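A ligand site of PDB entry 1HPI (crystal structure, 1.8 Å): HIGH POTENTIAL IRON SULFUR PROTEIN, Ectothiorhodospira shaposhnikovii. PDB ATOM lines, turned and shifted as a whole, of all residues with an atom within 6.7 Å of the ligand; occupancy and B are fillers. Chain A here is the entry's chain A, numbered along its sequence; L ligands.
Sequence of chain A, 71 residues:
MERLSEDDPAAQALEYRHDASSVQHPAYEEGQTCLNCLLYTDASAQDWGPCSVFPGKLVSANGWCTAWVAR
FE3 of the ligand is bound by SG of Cys 51, at 2.2 Å.
N of Cys 65 lies close to S3 of the ligand (3.6 Å).
The side-chain sulfur (SG) of Cys 65 is bound to an iron atom (FE4) of the ligand (2.2 Å).
The side-chain sulfur (SG) of Cys 37 binds an iron atom (FE2) of the ligand.
FE1 of the ligand is bound by SG of Cys 34, at 2.3 Å.
Tyr 16 touches the ligand (CD1 to S2, 3.8 Å).
CD1 of Leu 39 touches S1 of the ligand, 3.9 Å away.
Tyr 40 touches the ligand (CB to S4, 3.7 Å).
CG1 of Val 53 touches S1 of the ligand (3.7 Å).
CE2 of Phe 54 touches S2 of the ligand, 3.8 Å away.
Trp 64 touches the ligand.
CB of Ala 67 touches S1 of the ligand, at 3.9 Å.
Trp 68 touches the ligand.
Hydrophobic or aromatic side chains that line the ligand: Tyr 16, Leu 39, Tyr 40, Val 53, Phe 54, Ala 67 and Trp 68.
SG of Cys 51 sits close to N of Val 53, 3.5 Å away.
SG of Cys 65 lies close to N of Ala 67, 3.3 Å away.
SG of Cys 37 lies close to N of Val 69, 3.6 Å away.
N of Trp 64 lies close to SG of Cys 34 (3.8 Å).
The backbone NH (N) of Cys 34 sits at hydrogen-bond distance from the backbone carbonyl oxygen (O) of Gly 63 (3.0 Å).
O of Ser 60 sits close to SG of Cys 34 (3.2 Å).
NE1 of Trp 68 is in hydrogen-bond range of OD1 of Asn 36.
N of Ser 52 sits at hydrogen-bond distance from O of Leu 39, at 2.9 Å.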
ATOM      1  N   LEU A   4      -3.323  -4.088 -17.091  1.00  0.00           N
ATOM      2  CA  LEU A   4      -2.283  -4.603 -17.981  1.00  0.00           C
ATOM      3  C   LEU A   4      -1.660  -5.854 -17.345  1.00  0.00           C
ATOM      4  O   LEU A   4      -1.511  -5.930 -16.127  1.00  0.00           O
ATOM      5  CB  LEU A   4      -1.151  -3.548 -17.979  1.00  0.00           C
ATOM      6  CG  LEU A   4       0.062  -3.868 -18.846  1.00  0.00           C
ATOM      7  CD1 LEU A   4      -0.333  -3.998 -20.312  1.00  0.00           C
ATOM      8  CD2 LEU A   4       1.091  -2.757 -18.676  1.00  0.00           C
ATOM      9  N   LEU A  14       8.174  -2.692 -23.071  1.00  0.00           N
ATOM     10  CA  LEU A  14       8.624  -1.610 -22.203  1.00  0.00           C
ATOM     11  C   LEU A  14       9.179  -2.126 -20.877  1.00  0.00           C
ATOM     12  O   LEU A  14       9.424  -1.356 -19.962  1.00  0.00           O
ATOM     13  CB  LEU A  14       7.476  -0.625 -21.972  1.00  0.00           C
ATOM     14  CG  LEU A  14       7.153   0.128 -23.264  1.00  0.00           C
ATOM     15  CD1 LEU A  14       5.997   1.082 -23.036  1.00  0.00           C
ATOM     16  CD2 LEU A  14       8.390   0.882 -23.765  1.00  0.00           C
ATOM     17  N   TYR A  16       7.854  -3.589 -18.520  1.00  0.00           N
ATOM     18  CA  TYR A  16       6.994  -3.210 -17.425  1.00  0.00           C
ATOM     19  C   TYR A  16       6.876  -4.231 -16.309  1.00  0.00           C
ATOM     20  O   TYR A  16       6.826  -5.424 -16.541  1.00  0.00           O
ATOM     21  CB  TYR A  16       5.581  -2.905 -17.989  1.00  0.00           C
ATOM     22  CG  TYR A  16       4.511  -2.807 -16.923  1.00  0.00           C
ATOM     23  CD1 TYR A  16       4.253  -1.572 -16.325  1.00  0.00           C
ATOM     24  CD2 TYR A  16       3.762  -3.907 -16.511  1.00  0.00           C
ATOM     25  CE1 TYR A  16       3.278  -1.438 -15.335  1.00  0.00           C
ATOM     26  CE2 TYR A  16       2.778  -3.801 -15.533  1.00  0.00           C
ATOM     27  CZ  TYR A  16       2.551  -2.562 -14.943  1.00  0.00           C
ATOM     28  OH  TYR A  16       1.586  -2.424 -13.962  1.00  0.00           O
ATOM     29  N   THR A  33       8.340   5.334  -9.906  1.00  0.00           N
ATOM     30  CA  THR A  33       7.165   4.481  -9.959  1.00  0.00           C
ATOM     31  C   THR A  33       6.159   5.113 -10.908  1.00  0.00           C
ATOM     32  O   THR A  33       6.282   6.291 -11.281  1.00  0.00           O
ATOM     33  CB  THR A  33       6.463   4.285  -8.589  1.00  0.00           C
ATOM     34  OG1 THR A  33       5.976   5.528  -8.153  1.00  0.00           O
ATOM     35  CG2 THR A  33       7.402   3.681  -7.558  1.00  0.00           C
ATOM     36  N   CYS A  34       5.134   4.339 -11.277  1.00  0.00           N
ATOM     37  CA  CYS A  34       4.128   4.860 -12.162  1.00  0.00           C
ATOM     38  C   CYS A  34       3.504   6.072 -11.477  1.00  0.00           C
ATOM     39  O   CYS A  34       3.227   7.089 -12.099  1.00  0.00           O
ATOM     40  CB  CYS A  34       3.025   3.826 -12.457  1.00  0.00           C
ATOM     41  SG  CYS A  34       3.635   2.454 -13.445  1.00  0.00           S
ATOM     42  N   LEU A  35       3.297   5.931 -10.175  1.00  0.00           N
ATOM     43  CA  LEU A  35       2.710   6.999  -9.393  1.00  0.00           C
ATOM     44  C   LEU A  35       3.377   8.357  -9.599  1.00  0.00           C
ATOM     45  O   LEU A  35       2.699   9.384  -9.648  1.00  0.00           O
ATOM     46  CB  LEU A  35       2.528   6.615  -7.907  1.00  0.00           C
ATOM     47  CG  LEU A  35       1.574   7.535  -7.131  1.00  0.00           C
ATOM     48  CD1 LEU A  35       0.183   7.575  -7.756  1.00  0.00           C
ATOM     49  CD2 LEU A  35       1.470   7.026  -5.701  1.00  0.00           C
ATOM     50  N   ASN A  36       4.709   8.390  -9.735  1.00  0.00           N
ATOM     51  CA  ASN A  36       5.348   9.671  -9.940  1.00  0.00           C
ATOM     52  C   ASN A  36       5.794   9.894 -11.389  1.00  0.00           C
ATOM     53  O   ASN A  36       6.663  10.719 -11.688  1.00  0.00           O
ATOM     54  CB  ASN A  36       6.496   9.900  -8.941  1.00  0.00           C
ATOM     55  CG  ASN A  36       7.562   8.817  -8.967  1.00  0.00           C
ATOM     56  OD1 ASN A  36       7.752   8.113  -9.960  1.00  0.00           O
ATOM     57  ND2 ASN A  36       8.290   8.700  -7.861  1.00  0.00           N
ATOM     58  N   CYS A  37       5.187   9.146 -12.306  1.00  0.00           N
ATOM     59  CA  CYS A  37       5.493   9.239 -13.718  1.00  0.00           C
ATOM     60  C   CYS A  37       4.563  10.206 -14.442  1.00  0.00           C
ATOM     61  O   CYS A  37       3.358  10.172 -14.256  1.00  0.00           O
ATOM     62  CB  CYS A  37       5.379   7.846 -14.379  1.00  0.00           C
ATOM     63  SG  CYS A  37       5.714   7.841 -16.163  1.00  0.00           S
ATOM     64  N   LEU A  38       5.119  11.058 -15.288  1.00  0.00           N
ATOM     65  CA  LEU A  38       4.331  12.013 -16.041  1.00  0.00           C
ATOM     66  C   LEU A  38       3.226  11.362 -16.894  1.00  0.00           C
ATOM     67  O   LEU A  38       2.180  11.976 -17.097  1.00  0.00           O
ATOM     68  CB  LEU A  38       5.317  12.747 -16.963  1.00  0.00           C
ATOM     69  CG  LEU A  38       4.678  13.781 -17.870  1.00  0.00           C
ATOM     70  CD1 LEU A  38       4.105  14.900 -17.024  1.00  0.00           C
ATOM     71  CD2 LEU A  38       5.767  14.362 -18.771  1.00  0.00           C
ATOM     72  N   LEU A  39       3.417  10.129 -17.398  1.00  0.00           N
ATOM     73  CA  LEU A  39       2.443   9.429 -18.241  1.00  0.00           C
ATOM     74  C   LEU A  39       1.268   8.772 -17.515  1.00  0.00           C
ATOM     75  O   LEU A  39       0.334   8.254 -18.133  1.00  0.00           O
ATOM     76  CB  LEU A  39       3.104   8.498 -19.277  1.00  0.00           C
ATOM     77  CG  LEU A  39       4.298   9.142 -19.996  1.00  0.00           C
ATOM     78  CD1 LEU A  39       4.889   8.179 -21.016  1.00  0.00           C
ATOM     79  CD2 LEU A  39       3.897  10.444 -20.674  1.00  0.00           C
ATOM     80  N   TYR A  40       1.345   8.807 -16.181  1.00  0.00           N
ATOM     81  CA  TYR A  40       0.327   8.245 -15.289  1.00  0.00           C
ATOM     82  C   TYR A  40      -0.604   9.417 -15.090  1.00  0.00           C
ATOM     83  O   TYR A  40      -0.364  10.334 -14.299  1.00  0.00           O
ATOM     84  CB  TYR A  40       0.950   7.766 -13.967  1.00  0.00           C
ATOM     85  CG  TYR A  40       0.112   6.881 -13.075  1.00  0.00           C
ATOM     86  CD1 TYR A  40      -0.199   5.557 -13.396  1.00  0.00           C
ATOM     87  CD2 TYR A  40      -0.368   7.399 -11.871  1.00  0.00           C
ATOM     88  CE1 TYR A  40      -0.968   4.761 -12.530  1.00  0.00           C
ATOM     89  CE2 TYR A  40      -1.138   6.625 -11.007  1.00  0.00           C
ATOM     90  CZ  TYR A  40      -1.438   5.302 -11.327  1.00  0.00           C
ATOM     91  OH  TYR A  40      -2.186   4.517 -10.487  1.00  0.00           O
ATOM     92  N   THR A  41      -1.670   9.357 -15.877  1.00  0.00           N
ATOM     93  CA  THR A  41      -2.660  10.394 -15.918  1.00  0.00           C
ATOM     94  C   THR A  41      -3.410  10.836 -14.696  1.00  0.00           C
ATOM     95  O   THR A  41      -3.695  12.010 -14.545  1.00  0.00           O
ATOM     96  CB  THR A  41      -3.414  10.520 -17.239  1.00  0.00           C
ATOM     97  OG1 THR A  41      -4.235   9.394 -17.370  1.00  0.00           O
ATOM     98  CG2 THR A  41      -2.414  10.580 -18.386  1.00  0.00           C
ATOM     99  N   PRO A  50      -4.705   4.751 -15.318  1.00  0.00           N
ATOM    100  CA  PRO A  50      -4.358   4.822 -16.725  1.00  0.00           C
ATOM    101  C   PRO A  50      -2.964   5.369 -16.954  1.00  0.00           C
ATOM    102  O   PRO A  50      -2.380   6.107 -16.151  1.00  0.00           O
ATOM    103  CB  PRO A  50      -5.405   5.755 -17.351  1.00  0.00           C
ATOM    104  CG  PRO A  50      -6.165   6.410 -16.206  1.00  0.00           C
ATOM    105  CD  PRO A  50      -5.868   5.608 -14.956  1.00  0.00           C
ATOM    106  N   CYS A  51      -2.432   4.995 -18.108  1.00  0.00           N
ATOM    107  CA  CYS A  51      -1.107   5.395 -18.573  1.00  0.00           C
ATOM    108  C   CYS A  51      -1.174   5.737 -20.069  1.00  0.00           C
ATOM    109  O   CYS A  51      -1.636   4.917 -20.866  1.00  0.00           O
ATOM    110  CB  CYS A  51      -0.081   4.282 -18.311  1.00  0.00           C
ATOM    111  SG  CYS A  51       1.483   4.623 -19.163  1.00  0.00           S
ATOM    112  N   SER A  52      -0.718   6.915 -20.477  1.00  0.00           N
ATOM    113  CA  SER A  52      -0.753   7.342 -21.883  1.00  0.00           C
ATOM    114  C   SER A  52      -0.096   6.398 -22.859  1.00  0.00           C
ATOM    115  O   SER A  52      -0.514   6.281 -24.008  1.00  0.00           O
ATOM    116  CB  SER A  52      -0.070   8.688 -22.027  1.00  0.00           C
ATOM    117  OG  SER A  52      -0.748   9.538 -21.144  1.00  0.00           O
ATOM    118  N   VAL A  53       0.935   5.729 -22.409  1.00  0.00           N
ATOM    119  CA  VAL A  53       1.615   4.816 -23.296  1.00  0.00           C
ATOM    120  C   VAL A  53       0.971   3.448 -23.416  1.00  0.00           C
ATOM    121  O   VAL A  53       1.403   2.650 -24.250  1.00  0.00           O
ATOM    122  CB  VAL A  53       3.136   4.891 -23.134  1.00  0.00           C
ATOM    123  CG1 VAL A  53       3.638   4.084 -21.950  1.00  0.00           C
ATOM    124  CG2 VAL A  53       3.868   4.467 -24.404  1.00  0.00           C
ATOM    125  N   PHE A  54      -0.070   3.156 -22.612  1.00  0.00           N
ATOM    126  CA  PHE A  54      -0.772   1.880 -22.645  1.00  0.00           C
ATOM    127  C   PHE A  54      -2.267   2.128 -22.751  1.00  0.00           C
ATOM    128  O   PHE A  54      -3.018   1.918 -21.811  1.00  0.00           O
ATOM    129  CB  PHE A  54      -0.511   1.123 -21.326  1.00  0.00           C
ATOM    130  CG  PHE A  54       0.856   0.487 -21.264  1.00  0.00           C
ATOM    131  CD1 PHE A  54       1.094  -0.630 -22.053  1.00  0.00           C
ATOM    132  CD2 PHE A  54       1.879   0.962 -20.443  1.00  0.00           C
ATOM    133  CE1 PHE A  54       2.336  -1.284 -22.048  1.00  0.00           C
ATOM    134  CE2 PHE A  54       3.119   0.323 -20.421  1.00  0.00           C
ATOM    135  CZ  PHE A  54       3.348  -0.800 -21.224  1.00  0.00           C
ATOM    136  N   VAL A  59      -2.446   0.536 -15.180  1.00  0.00           N
ATOM    137  CA  VAL A  59      -1.129   0.073 -14.749  1.00  0.00           C
ATOM    138  C   VAL A  59      -1.038   0.196 -13.228  1.00  0.00           C
ATOM    139  O   VAL A  59      -1.804   0.958 -12.622  1.00  0.00           O
ATOM    140  CB  VAL A  59       0.030   0.783 -15.423  1.00  0.00           C
ATOM    141  CG1 VAL A  59      -0.121   0.632 -16.937  1.00  0.00           C
ATOM    142  CG2 VAL A  59       0.071   2.245 -15.029  1.00  0.00           C
ATOM    143  N   SER A  60      -0.125  -0.549 -12.632  1.00  0.00           N
ATOM    144  CA  SER A  60       0.084  -0.515 -11.193  1.00  0.00           C
ATOM    145  C   SER A  60       0.736   0.779 -10.724  1.00  0.00           C
ATOM    146  O   SER A  60       1.784   1.172 -11.239  1.00  0.00           O
ATOM    147  CB  SER A  60       0.966  -1.708 -10.831  1.00  0.00           C
ATOM    148  OG  SER A  60       1.381  -1.592  -9.488  1.00  0.00           O
ATOM    149  N   GLY A  63       4.263   0.316 -10.057  1.00  0.00           N
ATOM    150  CA  GLY A  63       5.048  -0.276 -11.144  1.00  0.00           C
ATOM    151  C   GLY A  63       6.100   0.632 -11.787  1.00  0.00           C
ATOM    152  O   GLY A  63       6.444   1.694 -11.267  1.00  0.00           O
ATOM    153  N   TRP A  64       6.604   0.177 -12.932  1.00  0.00           N
ATOM    154  CA  TRP A  64       7.626   0.915 -13.667  1.00  0.00           C
ATOM    155  C   TRP A  64       7.810   0.320 -15.049  1.00  0.00           C
ATOM    156  O   TRP A  64       7.536  -0.856 -15.244  1.00  0.00           O
ATOM    157  CB  TRP A  64       8.973   0.749 -12.922  1.00  0.00           C
ATOM    158  CG  TRP A  64      10.104   1.551 -13.506  1.00  0.00           C
ATOM    159  CD1 TRP A  64      10.444   2.814 -13.165  1.00  0.00           C
ATOM    160  CD2 TRP A  64      11.047   1.138 -14.502  1.00  0.00           C
ATOM    161  NE1 TRP A  64      11.526   3.230 -13.896  1.00  0.00           N
ATOM    162  CE2 TRP A  64      11.924   2.225 -14.728  1.00  0.00           C
ATOM    163  CE3 TRP A  64      11.222  -0.026 -15.237  1.00  0.00           C
ATOM    164  CZ2 TRP A  64      12.973   2.143 -15.649  1.00  0.00           C
ATOM    165  CZ3 TRP A  64      12.251  -0.102 -16.147  1.00  0.00           C
ATOM    166  CH2 TRP A  64      13.117   0.968 -16.358  1.00  0.00           C
ATOM    167  N   CYS A  65       8.284   1.112 -15.999  1.00  0.00           N
ATOM    168  CA  CYS A  65       8.562   0.662 -17.349  1.00  0.00           C
ATOM    169  C   CYS A  65       9.623   1.616 -17.866  1.00  0.00           C
ATOM    170  O   CYS A  65       9.871   2.661 -17.261  1.00  0.00           O
ATOM    171  CB  CYS A  65       7.348   0.530 -18.303  1.00  0.00           C
ATOM    172  SG  CYS A  65       6.854   2.097 -19.064  1.00  0.00           S
ATOM    173  N   THR A  66      10.242   1.253 -18.979  1.00  0.00           N
ATOM    174  CA  THR A  66      11.294   2.069 -19.583  1.00  0.00           C
ATOM    175  C   THR A  66      10.873   3.459 -20.022  1.00  0.00           C
ATOM    176  O   THR A  66      11.725   4.335 -20.237  1.00  0.00           O
ATOM    177  CB  THR A  66      12.055   1.317 -20.703  1.00  0.00           C
ATOM    178  OG1 THR A  66      11.155   1.031 -21.765  1.00  0.00           O
ATOM    179  CG2 THR A  66      12.699   0.042 -20.194  1.00  0.00           C
ATOM    180  N   ALA A  67       9.564   3.671 -20.175  1.00  0.00           N
ATOM    181  CA  ALA A  67       9.072   4.977 -20.576  1.00  0.00           C
ATOM    182  C   ALA A  67       8.922   5.903 -19.374  1.00  0.00           C
ATOM    183  O   ALA A  67       8.418   7.015 -19.508  1.00  0.00           O
ATOM    184  CB  ALA A  67       7.798   4.896 -21.395  1.00  0.00           C
ATOM    185  N   TRP A  68       9.343   5.479 -18.192  1.00  0.00           N
ATOM    186  CA  TRP A  68       9.227   6.344 -17.022  1.00  0.00           C
ATOM    187  C   TRP A  68       9.884   7.702 -17.228  1.00  0.00           C
ATOM    188  O   TRP A  68      11.016   7.813 -17.700  1.00  0.00           O
ATOM    189  CB  TRP A  68       9.809   5.702 -15.756  1.00  0.00           C
ATOM    190  CG  TRP A  68       9.550   6.558 -14.555  1.00  0.00           C
ATOM    191  CD1 TRP A  68       8.493   6.448 -13.722  1.00  0.00           C
ATOM    192  CD2 TRP A  68      10.338   7.641 -14.077  1.00  0.00           C
ATOM    193  NE1 TRP A  68       8.567   7.409 -12.740  1.00  0.00           N
ATOM    194  CE2 TRP A  68       9.692   8.154 -12.938  1.00  0.00           C
ATOM    195  CE3 TRP A  68      11.543   8.230 -14.494  1.00  0.00           C
ATOM    196  CZ2 TRP A  68      10.213   9.233 -12.217  1.00  0.00           C
ATOM    197  CZ3 TRP A  68      12.054   9.300 -13.777  1.00  0.00           C
ATOM    198  CH2 TRP A  68      11.390   9.798 -12.656  1.00  0.00           C
ATOM    199  N   VAL A  69       9.165   8.747 -16.841  1.00  0.00           N
ATOM    200  CA  VAL A  69       9.644  10.118 -16.944  1.00  0.00           C
ATOM    201  C   VAL A  69       9.068  10.927 -15.780  1.00  0.00           C
ATOM    202  O   VAL A  69       7.884  10.825 -15.447  1.00  0.00           O
ATOM    203  CB  VAL A  69       9.485  10.694 -18.362  1.00  0.00           C
ATOM    204  CG1 VAL A  69       8.030  10.692 -18.782  1.00  0.00           C
ATOM    205  CG2 VAL A  69      10.035  12.104 -18.500  1.00  0.00           C
HETATM  206 FE1  LIG L   1       4.183   3.450 -15.388  1.00  0.00          FE
HETATM  207 FE2  LIG L   1       5.121   5.737 -16.565  1.00  0.00          FE
HETATM  208 FE3  LIG L   1       3.129   4.266 -17.732  1.00  0.00          FE
HETATM  209 FE4  LIG L   1       5.665   3.255 -17.591  1.00  0.00          FE
HETATM  210  S1  LIG L   1       5.016   5.117 -18.685  1.00  0.00           S
HETATM  211  S2  LIG L   1       3.760   2.146 -17.131  1.00  0.00           S
HETATM  212  S3  LIG L   1       6.349   4.091 -15.663  1.00  0.00           S
HETATM  213  S4  LIG L   1       3.040   5.311 -15.734  1.00  0.00           S
